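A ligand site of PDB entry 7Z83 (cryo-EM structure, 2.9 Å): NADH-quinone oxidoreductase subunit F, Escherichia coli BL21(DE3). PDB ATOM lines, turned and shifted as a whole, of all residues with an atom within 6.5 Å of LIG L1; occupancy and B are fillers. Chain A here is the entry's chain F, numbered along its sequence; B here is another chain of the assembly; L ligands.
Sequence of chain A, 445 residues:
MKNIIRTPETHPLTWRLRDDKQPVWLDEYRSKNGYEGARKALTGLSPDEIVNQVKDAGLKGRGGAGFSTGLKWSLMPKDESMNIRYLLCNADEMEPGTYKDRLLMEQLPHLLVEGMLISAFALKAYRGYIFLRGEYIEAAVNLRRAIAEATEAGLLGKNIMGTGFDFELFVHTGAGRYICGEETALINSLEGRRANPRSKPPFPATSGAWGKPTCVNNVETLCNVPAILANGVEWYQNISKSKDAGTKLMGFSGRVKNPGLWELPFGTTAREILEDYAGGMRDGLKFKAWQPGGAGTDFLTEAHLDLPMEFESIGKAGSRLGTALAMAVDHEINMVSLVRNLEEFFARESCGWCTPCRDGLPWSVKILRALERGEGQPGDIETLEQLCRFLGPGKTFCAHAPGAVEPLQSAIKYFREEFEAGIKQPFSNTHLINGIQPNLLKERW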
ATOM      1  N   ILE A 179      32.235 -18.588 -21.948  1.00  0.00           N
ATOM      2  CA  ILE A 179      32.175 -18.827 -23.393  1.00  0.00           C
ATOM      3  C   ILE A 179      32.926 -20.105 -23.777  1.00  0.00           C
ATOM      4  O   ILE A 179      32.695 -20.632 -24.868  1.00  0.00           O
ATOM      5  CB  ILE A 179      32.711 -17.588 -24.136  1.00  0.00           C
ATOM      6  CG1 ILE A 179      32.273 -17.585 -25.610  1.00  0.00           C
ATOM      7  CG2 ILE A 179      34.214 -17.489 -24.021  1.00  0.00           C
ATOM      8  CD1 ILE A 179      30.813 -17.934 -25.824  1.00  0.00           C
ATOM      9  N   ALA A 195      39.320 -18.060 -26.189  1.00  0.00           N
ATOM     10  CA  ALA A 195      38.143 -18.887 -26.462  1.00  0.00           C
ATOM     11  C   ALA A 195      37.080 -18.122 -27.251  1.00  0.00           C
ATOM     12  O   ALA A 195      35.924 -17.991 -26.849  1.00  0.00           O
ATOM     13  CB  ALA A 195      37.577 -19.443 -25.160  1.00  0.00           C
ATOM     14  N   ASN A 196      37.491 -17.614 -28.394  1.00  0.00           N
ATOM     15  CA  ASN A 196      36.535 -17.100 -29.359  1.00  0.00           C
ATOM     16  C   ASN A 196      35.965 -18.258 -30.176  1.00  0.00           C
ATOM     17  O   ASN A 196      36.729 -19.138 -30.596  1.00  0.00           O
ATOM     18  CB  ASN A 196      37.180 -16.078 -30.284  1.00  0.00           C
ATOM     19  CG  ASN A 196      37.656 -14.838 -29.549  1.00  0.00           C
ATOM     20  OD1 ASN A 196      38.854 -14.585 -29.455  1.00  0.00           O
ATOM     21  ND2 ASN A 196      36.719 -14.067 -29.020  1.00  0.00           N
ATOM     22  N   PRO A 197      34.664 -18.299 -30.407  1.00  0.00           N
ATOM     23  CA  PRO A 197      34.072 -19.366 -31.215  1.00  0.00           C
ATOM     24  C   PRO A 197      34.495 -19.268 -32.673  1.00  0.00           C
ATOM     25  O   PRO A 197      35.143 -18.315 -33.117  1.00  0.00           O
ATOM     26  CB  PRO A 197      32.565 -19.164 -31.060  1.00  0.00           C
ATOM     27  CG  PRO A 197      32.404 -17.800 -30.500  1.00  0.00           C
ATOM     28  CD  PRO A 197      33.627 -17.493 -29.726  1.00  0.00           C
ATOM     29  N   GLU A 349      30.482 -11.980 -19.452  1.00  0.00           N
ATOM     30  CA  GLU A 349      30.989 -13.240 -19.975  1.00  0.00           C
ATOM     31  C   GLU A 349      30.999 -13.257 -21.501  1.00  0.00           C
ATOM     32  O   GLU A 349      31.159 -14.322 -22.097  1.00  0.00           O
ATOM     33  CB  GLU A 349      30.169 -14.405 -19.439  1.00  0.00           C
ATOM     34  CG  GLU A 349      30.363 -14.610 -17.952  1.00  0.00           C
ATOM     35  CD  GLU A 349      31.804 -14.830 -17.568  1.00  0.00           C
ATOM     36  OE1 GLU A 349      32.463 -15.682 -18.209  1.00  0.00           O
ATOM     37  OE2 GLU A 349      32.294 -14.156 -16.637  1.00  0.00           O
ATOM     38  N   SER A 350      30.822 -12.108 -22.128  1.00  0.00           N
ATOM     39  CA  SER A 350      31.041 -11.971 -23.554  1.00  0.00           C
ATOM     40  C   SER A 350      32.510 -12.224 -23.880  1.00  0.00           C
ATOM     41  O   SER A 350      33.400 -11.928 -23.081  1.00  0.00           O
ATOM     42  CB  SER A 350      30.623 -10.580 -24.018  1.00  0.00           C
ATOM     43  OG  SER A 350      31.183 -10.264 -25.283  1.00  0.00           O
ATOM     44  N   CYS A 351      32.763 -12.801 -25.042  1.00  0.00           N
ATOM     45  CA  CYS A 351      34.134 -13.053 -25.472  1.00  0.00           C
ATOM     46  C   CYS A 351      34.744 -11.865 -26.201  1.00  0.00           C
ATOM     47  O   CYS A 351      35.971 -11.821 -26.347  1.00  0.00           O
ATOM     48  CB  CYS A 351      34.189 -14.295 -26.351  1.00  0.00           C
ATOM     49  SG  CYS A 351      33.951 -13.967 -28.094  1.00  0.00           S
ATOM     50  N   GLY A 352      33.928 -10.917 -26.648  1.00  0.00           N
ATOM     51  CA  GLY A 352      34.439  -9.715 -27.279  1.00  0.00           C
ATOM     52  C   GLY A 352      34.664  -9.796 -28.772  1.00  0.00           C
ATOM     53  O   GLY A 352      35.178  -8.831 -29.343  1.00  0.00           O
ATOM     54  N   TRP A 353      34.315 -10.906 -29.415  1.00  0.00           N
ATOM     55  CA  TRP A 353      34.603 -11.061 -30.833  1.00  0.00           C
ATOM     56  C   TRP A 353      33.728 -10.150 -31.684  1.00  0.00           C
ATOM     57  O   TRP A 353      34.224  -9.453 -32.579  1.00  0.00           O
ATOM     58  CB  TRP A 353      34.436 -12.516 -31.256  1.00  0.00           C
ATOM     59  CG  TRP A 353      34.706 -12.786 -32.699  1.00  0.00           C
ATOM     60  CD1 TRP A 353      33.807 -13.182 -33.634  1.00  0.00           C
ATOM     61  CD2 TRP A 353      35.966 -12.678 -33.369  1.00  0.00           C
ATOM     62  NE1 TRP A 353      34.416 -13.332 -34.853  1.00  0.00           N
ATOM     63  CE2 TRP A 353      35.751 -13.023 -34.718  1.00  0.00           C
ATOM     64  CE3 TRP A 353      37.253 -12.307 -32.970  1.00  0.00           C
ATOM     65  CZ2 TRP A 353      36.763 -13.020 -35.658  1.00  0.00           C
ATOM     66  CZ3 TRP A 353      38.256 -12.315 -33.909  1.00  0.00           C
ATOM     67  CH2 TRP A 353      38.017 -12.666 -35.239  1.00  0.00           C
ATOM     68  N   CYS A 354      32.427 -10.129 -31.431  1.00  0.00           N
ATOM     69  CA  CYS A 354      31.498  -9.515 -32.359  1.00  0.00           C
ATOM     70  C   CYS A 354      30.701  -8.386 -31.707  1.00  0.00           C
ATOM     71  O   CYS A 354      30.370  -8.428 -30.521  1.00  0.00           O
ATOM     72  CB  CYS A 354      30.578 -10.562 -32.992  1.00  0.00           C
ATOM     73  SG  CYS A 354      29.185 -11.140 -32.043  1.00  0.00           S
ATOM     74  N   THR A 355      30.394  -7.380 -32.532  1.00  0.00           N
ATOM     75  CA  THR A 355      29.867  -6.096 -32.053  1.00  0.00           C
ATOM     76  C   THR A 355      28.535  -6.151 -31.310  1.00  0.00           C
ATOM     77  O   THR A 355      28.425  -5.477 -30.275  1.00  0.00           O
ATOM     78  CB  THR A 355      29.805  -5.125 -33.240  1.00  0.00           C
ATOM     79  OG1 THR A 355      31.109  -4.947 -33.792  1.00  0.00           O
ATOM     80  CG2 THR A 355      29.240  -3.769 -32.832  1.00  0.00           C
ATOM     81  N   PRO A 356      27.483  -6.862 -31.767  1.00  0.00           N
ATOM     82  CA  PRO A 356      26.188  -6.739 -31.073  1.00  0.00           C
ATOM     83  C   PRO A 356      26.204  -7.166 -29.618  1.00  0.00           C
ATOM     84  O   PRO A 356      25.788  -6.399 -28.754  1.00  0.00           O
ATOM     85  CB  PRO A 356      25.254  -7.622 -31.915  1.00  0.00           C
ATOM     86  CG  PRO A 356      25.859  -7.618 -33.229  1.00  0.00           C
ATOM     87  CD  PRO A 356      27.305  -7.712 -32.963  1.00  0.00           C
ATOM     88  N   CYS A 357      26.743  -8.354 -29.318  1.00  0.00           N
ATOM     89  CA  CYS A 357      26.848  -8.792 -27.926  1.00  0.00           C
ATOM     90  C   CYS A 357      27.781  -7.885 -27.140  1.00  0.00           C
ATOM     91  O   CYS A 357      27.368  -7.277 -26.143  1.00  0.00           O
ATOM     92  CB  CYS A 357      27.306 -10.249 -27.917  1.00  0.00           C
ATOM     93  SG  CYS A 357      28.105 -10.975 -26.486  1.00  0.00           S
ATOM     94  N   ARG A 358      29.005  -7.676 -27.654  1.00  0.00           N
ATOM     95  CA  ARG A 358      30.058  -6.968 -26.919  1.00  0.00           C
ATOM     96  C   ARG A 358      29.678  -5.523 -26.622  1.00  0.00           C
ATOM     97  O   ARG A 358      29.980  -5.008 -25.539  1.00  0.00           O
ATOM     98  CB  ARG A 358      31.362  -7.022 -27.719  1.00  0.00           C
ATOM     99  CG  ARG A 358      32.310  -5.849 -27.521  1.00  0.00           C
ATOM    100  CD  ARG A 358      33.474  -5.853 -28.500  1.00  0.00           C
ATOM    101  NE  ARG A 358      33.224  -4.963 -29.629  1.00  0.00           N
ATOM    102  CZ  ARG A 358      33.208  -5.355 -30.892  1.00  0.00           C
ATOM    103  NH1 ARG A 358      33.452  -6.611 -31.241  1.00  0.00           N
ATOM    104  NH2 ARG A 358      32.941  -4.460 -31.835  1.00  0.00           N
ATOM    105  N   LEU A 361      25.101  -5.653 -25.093  1.00  0.00           N
ATOM    106  CA  LEU A 361      24.780  -6.132 -23.751  1.00  0.00           C
ATOM    107  C   LEU A 361      25.143  -5.136 -22.646  1.00  0.00           C
ATOM    108  O   LEU A 361      24.343  -5.001 -21.697  1.00  0.00           O
ATOM    109  CB  LEU A 361      25.427  -7.511 -23.520  1.00  0.00           C
ATOM    110  CG  LEU A 361      24.792  -8.668 -24.289  1.00  0.00           C
ATOM    111  CD1 LEU A 361      25.438  -9.983 -23.896  1.00  0.00           C
ATOM    112  CD2 LEU A 361      23.297  -8.719 -24.063  1.00  0.00           C
ATOM    113  N   THR A 396      24.426 -12.296 -34.377  1.00  0.00           N
ATOM    114  CA  THR A 396      25.710 -12.345 -33.693  1.00  0.00           C
ATOM    115  C   THR A 396      26.504 -13.545 -34.180  1.00  0.00           C
ATOM    116  O   THR A 396      25.986 -14.446 -34.847  1.00  0.00           O
ATOM    117  CB  THR A 396      25.519 -12.409 -32.174  1.00  0.00           C
ATOM    118  OG1 THR A 396      24.838 -13.624 -31.825  1.00  0.00           O
ATOM    119  CG2 THR A 396      24.686 -11.233 -31.705  1.00  0.00           C
ATOM    120  N   PHE A 397      27.795 -13.553 -33.831  1.00  0.00           N
ATOM    121  CA  PHE A 397      28.693 -14.591 -34.323  1.00  0.00           C
ATOM    122  C   PHE A 397      28.409 -15.941 -33.699  1.00  0.00           C
ATOM    123  O   PHE A 397      28.624 -16.971 -34.344  1.00  0.00           O
ATOM    124  CB  PHE A 397      30.138 -14.165 -34.075  1.00  0.00           C
ATOM    125  CG  PHE A 397      31.152 -15.051 -34.723  1.00  0.00           C
ATOM    126  CD1 PHE A 397      31.430 -14.911 -36.074  1.00  0.00           C
ATOM    127  CD2 PHE A 397      31.832 -16.010 -33.997  1.00  0.00           C
ATOM    128  CE1 PHE A 397      32.363 -15.720 -36.684  1.00  0.00           C
ATOM    129  CE2 PHE A 397      32.759 -16.823 -34.600  1.00  0.00           C
ATOM    130  CZ  PHE A 397      33.026 -16.674 -35.940  1.00  0.00           C
ATOM    131  N   CYS A 398      27.925 -15.973 -32.462  1.00  0.00           N
ATOM    132  CA  CYS A 398      27.588 -17.222 -31.792  1.00  0.00           C
ATOM    133  C   CYS A 398      26.268 -17.050 -31.061  1.00  0.00           C
ATOM    134  O   CYS A 398      25.662 -15.967 -31.083  1.00  0.00           O
ATOM    135  CB  CYS A 398      28.715 -17.668 -30.863  1.00  0.00           C
ATOM    136  SG  CYS A 398      28.617 -17.069 -29.177  1.00  0.00           S
ATOM    137  N   ALA A 399      25.817 -18.116 -30.402  1.00  0.00           N
ATOM    138  CA  ALA A 399      24.500 -18.154 -29.790  1.00  0.00           C
ATOM    139  C   ALA A 399      24.487 -17.691 -28.342  1.00  0.00           C
ATOM    140  O   ALA A 399      23.522 -17.973 -27.625  1.00  0.00           O
ATOM    141  CB  ALA A 399      23.917 -19.573 -29.889  1.00  0.00           C
ATOM    142  N   HIS A 400      25.525 -16.988 -27.900  1.00  0.00           N
ATOM    143  CA  HIS A 400      25.566 -16.500 -26.520  1.00  0.00           C
ATOM    144  C   HIS A 400      24.597 -15.338 -26.319  1.00  0.00           C
ATOM    145  O   HIS A 400      23.868 -15.294 -25.325  1.00  0.00           O
ATOM    146  CB  HIS A 400      27.000 -16.096 -26.168  1.00  0.00           C
ATOM    147  CG  HIS A 400      27.108 -15.164 -25.006  1.00  0.00           C
ATOM    148  ND1 HIS A 400      27.110 -13.797 -25.155  1.00  0.00           N
ATOM    149  CD2 HIS A 400      27.233 -15.404 -23.678  1.00  0.00           C
ATOM    150  CE1 HIS A 400      27.230 -13.238 -23.965  1.00  0.00           C
ATOM    151  NE2 HIS A 400      27.309 -14.183 -23.058  1.00  0.00           N
ATOM    152  N   ALA A 401      24.561 -14.403 -27.267  1.00  0.00           N
ATOM    153  CA  ALA A 401      23.693 -13.229 -27.190  1.00  0.00           C
ATOM    154  C   ALA A 401      22.202 -13.497 -27.395  1.00  0.00           C
ATOM    155  O   ALA A 401      21.392 -12.797 -26.781  1.00  0.00           O
ATOM    156  CB  ALA A 401      24.177 -12.170 -28.177  1.00  0.00           C
ATOM    157  N   PRO A 402      21.773 -14.435 -28.266  1.00  0.00           N
ATOM    158  CA  PRO A 402      20.339 -14.801 -28.232  1.00  0.00           C
ATOM    159  C   PRO A 402      19.888 -15.347 -26.892  1.00  0.00           C
ATOM    160  O   PRO A 402      18.794 -14.989 -26.406  1.00  0.00           O
ATOM    161  CB  PRO A 402      20.227 -15.863 -29.334  1.00  0.00           C
ATOM    162  CG  PRO A 402      21.269 -15.511 -30.284  1.00  0.00           C
ATOM    163  CD  PRO A 402      22.410 -14.982 -29.486  1.00  0.00           C
ATOM    164  N   HIS B 176      35.385  -9.085 -22.631  1.00  0.00           N
ATOM    165  CA  HIS B 176      34.075  -8.772 -23.194  1.00  0.00           C
ATOM    166  C   HIS B 176      33.971  -7.452 -23.957  1.00  0.00           C
ATOM    167  O   HIS B 176      33.680  -7.435 -25.154  1.00  0.00           O
ATOM    168  CB  HIS B 176      33.114  -8.749 -22.017  1.00  0.00           C
ATOM    169  CG  HIS B 176      33.752  -8.295 -20.734  1.00  0.00           C
ATOM    170  ND1 HIS B 176      33.865  -6.973 -20.390  1.00  0.00           N
ATOM    171  CD2 HIS B 176      34.354  -8.994 -19.736  1.00  0.00           C
ATOM    172  CE1 HIS B 176      34.487  -6.868 -19.226  1.00  0.00           C
ATOM    173  NE2 HIS B 176      34.798  -8.084 -18.813  1.00  0.00           N
HETATM  174 FE1  LIG L   1      29.835 -12.503 -30.291  1.00  0.00          FE
HETATM  175 FE2  LIG L   1      29.343 -12.493 -27.720  1.00  0.00          FE
HETATM  176 FE3  LIG L   1      29.474 -14.912 -29.005  1.00  0.00          FE
HETATM  177 FE4  LIG L   1      31.707 -13.573 -28.543  1.00  0.00          FE
HETATM  178  S1  LIG L   1      30.308 -14.419 -26.917  1.00  0.00           S
HETATM  179  S2  LIG L   1      31.073 -14.426 -30.588  1.00  0.00           S
HETATM  180  S3  LIG L   1      31.086 -11.365 -28.730  1.00  0.00           S
HETATM  181  S4  LIG L   1      27.900 -13.277 -29.323  1.00  0.00           S
HETATM  182  N1  LG2 L   2      27.430 -27.257 -23.624  1.00  0.00           N
HETATM  183  C1  LG2 L   2      27.906 -27.902 -22.511  1.00  0.00           C
HETATM  184  O1  LG2 L   2      27.820 -29.124 -22.440  1.00  0.00           O
HETATM  185  N2  LG2 L   2      28.454 -27.180 -21.477  1.00  0.00           N
HETATM  186  C2  LG2 L   2      28.542 -25.816 -21.574  1.00  0.00           C
HETATM  187  O2  LG2 L   2      29.039 -25.158 -20.661  1.00  0.00           O
HETATM  188  C3  LG2 L   2      28.078 -25.163 -22.702  1.00  0.00           C
HETATM  189  N3  LG2 L   2      28.153 -23.797 -22.795  1.00  0.00           N
HETATM  190  C4  LG2 L   2      27.690 -23.153 -23.913  1.00  0.00           C
HETATM  191  C5  LG2 L   2      27.782 -21.774 -23.984  1.00  0.00           C
HETATM  192  C6  LG2 L   2      27.324 -21.106 -25.099  1.00  0.00           C
HETATM  193  C7  LG2 L   2      27.437 -19.614 -25.158  1.00  0.00           C
HETATM  194  C8  LG2 L   2      26.763 -21.819 -26.151  1.00  0.00           C
HETATM  195  C9  LG2 L   2      26.242 -21.107 -27.372  1.00  0.00           C
HETATM  196  C10 LG2 L   2      26.665 -23.203 -26.073  1.00  0.00           C
HETATM  197  C11 LG2 L   2      27.130 -23.877 -24.956  1.00  0.00           C
HETATM  198  N4  LG2 L   2      27.043 -25.260 -24.869  1.00  0.00           N
HETATM  199  C12 LG2 L   2      27.513 -25.890 -23.738  1.00  0.00           C
HETATM  200  C13 LG2 L   2      26.440 -26.079 -25.974  1.00  0.00           C
HETATM  201  C14 LG2 L   2      27.548 -26.555 -26.924  1.00  0.00           C
HETATM  202  O3  LG2 L   2      27.682 -25.636 -27.988  1.00  0.00           O
HETATM  203  C15 LG2 L   2      27.267 -27.935 -27.505  1.00  0.00           C
HETATM  204  O4  LG2 L   2      25.942 -27.969 -27.975  1.00  0.00           O
HETATM  205  C16 LG2 L   2      27.457 -29.007 -26.432  1.00  0.00           C
HETATM  206  O5  LG2 L   2      28.564 -28.669 -25.632  1.00  0.00           O
HETATM  207  C17 LG2 L   2      27.663 -30.399 -27.001  1.00  0.00           C
HETATM  208  O6  LG2 L   2      26.542 -30.770 -27.760  1.00  0.00           O
HETATM  209  P1  LG2 L   2      25.595 -31.980 -27.266  1.00  0.00           P
HETATM  210  O7  LG2 L   2      24.384 -31.372 -26.613  1.00  0.00           O
HETATM  211  O8  LG2 L   2      25.183 -32.821 -28.444  1.00  0.00           O
HETATM  212  O9  LG2 L   2      26.327 -32.830 -26.268  1.00  0.00           O
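FE1 of LIG L1 is bound by SG of Cys 354 (2.3 Å).
SG of Cys 351 is bound to FE4 of LIG L1 (2.3 Å).
A sulfur (S3) of LIG L1 sits close to the backbone NH of Gly 352, 3.6 Å away.
FE3 of LIG L1 is bound by SG of Cys 398 (2.3 Å).
A sulfur (S3) of LIG L1 sits close to the side-chain hydroxyl (OG) of Ser 350 (3.6 Å).
S1 of LIG L1 sits close to N of Cys 351 (3.5 Å).
SG of Cys 357 is bound to FE2 of LIG L1 (2.3 Å).
A sulfur (S3) of LIG L1 sits close to the backbone NH (N) of Trp 353, 3.3 Å away.
A sulfur (S3) of LIG L1 lies close to the backbone NH of Cys 354, at 3.3 Å.
A ring nitrogen (ND1) of His 400 lies close to a sulfur (S1) of LIG L1 (3.7 Å).
The backbone NH (N) of Gly 352 is in hydrogen-bond range of the side-chain hydroxyl (OG) of Ser 350 (3.1 Å).
The side-chain amide nitrogen of Asn 196 sits close to the side-chain sulfur of Cys 351, at 2.9 Å.
The backbone NH (N) of His 400 lies close to the side-chain sulfur (SG) of Cys 398.
NH1 of Arg 358 sits at hydrogen-bond distance from O of Gly 352 (3.4 Å).
The side-chain sulfur (SG) of Cys 357 sits close to the side-chain hydroxyl (OG) of Ser 350, at 3.4 Å.
SG of Cys 351 lies close to N of Trp 353.
SG of Cys 354 sits close to N of Phe 397 (3.3 Å).
The backbone carbonyl oxygen (O) of Trp 353 sits at hydrogen-bond distance from the guanidinium group (NH1) of Arg 358 (3.2 Å).
Residues that only touch LIG L1: Phe 397 (3.6 Å), Pro 197 (3.6 Å), Ile 179 (3.7 Å) and Thr 396 (3.8 Å).
Hydrophobic or aromatic side chains that line LIG L1: Ile 179, Pro 197, Trp 353, Phe 397 and His 400.
The nearest printed residue that does not touch LIG L1 is Ala 401 (4.05 Å).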
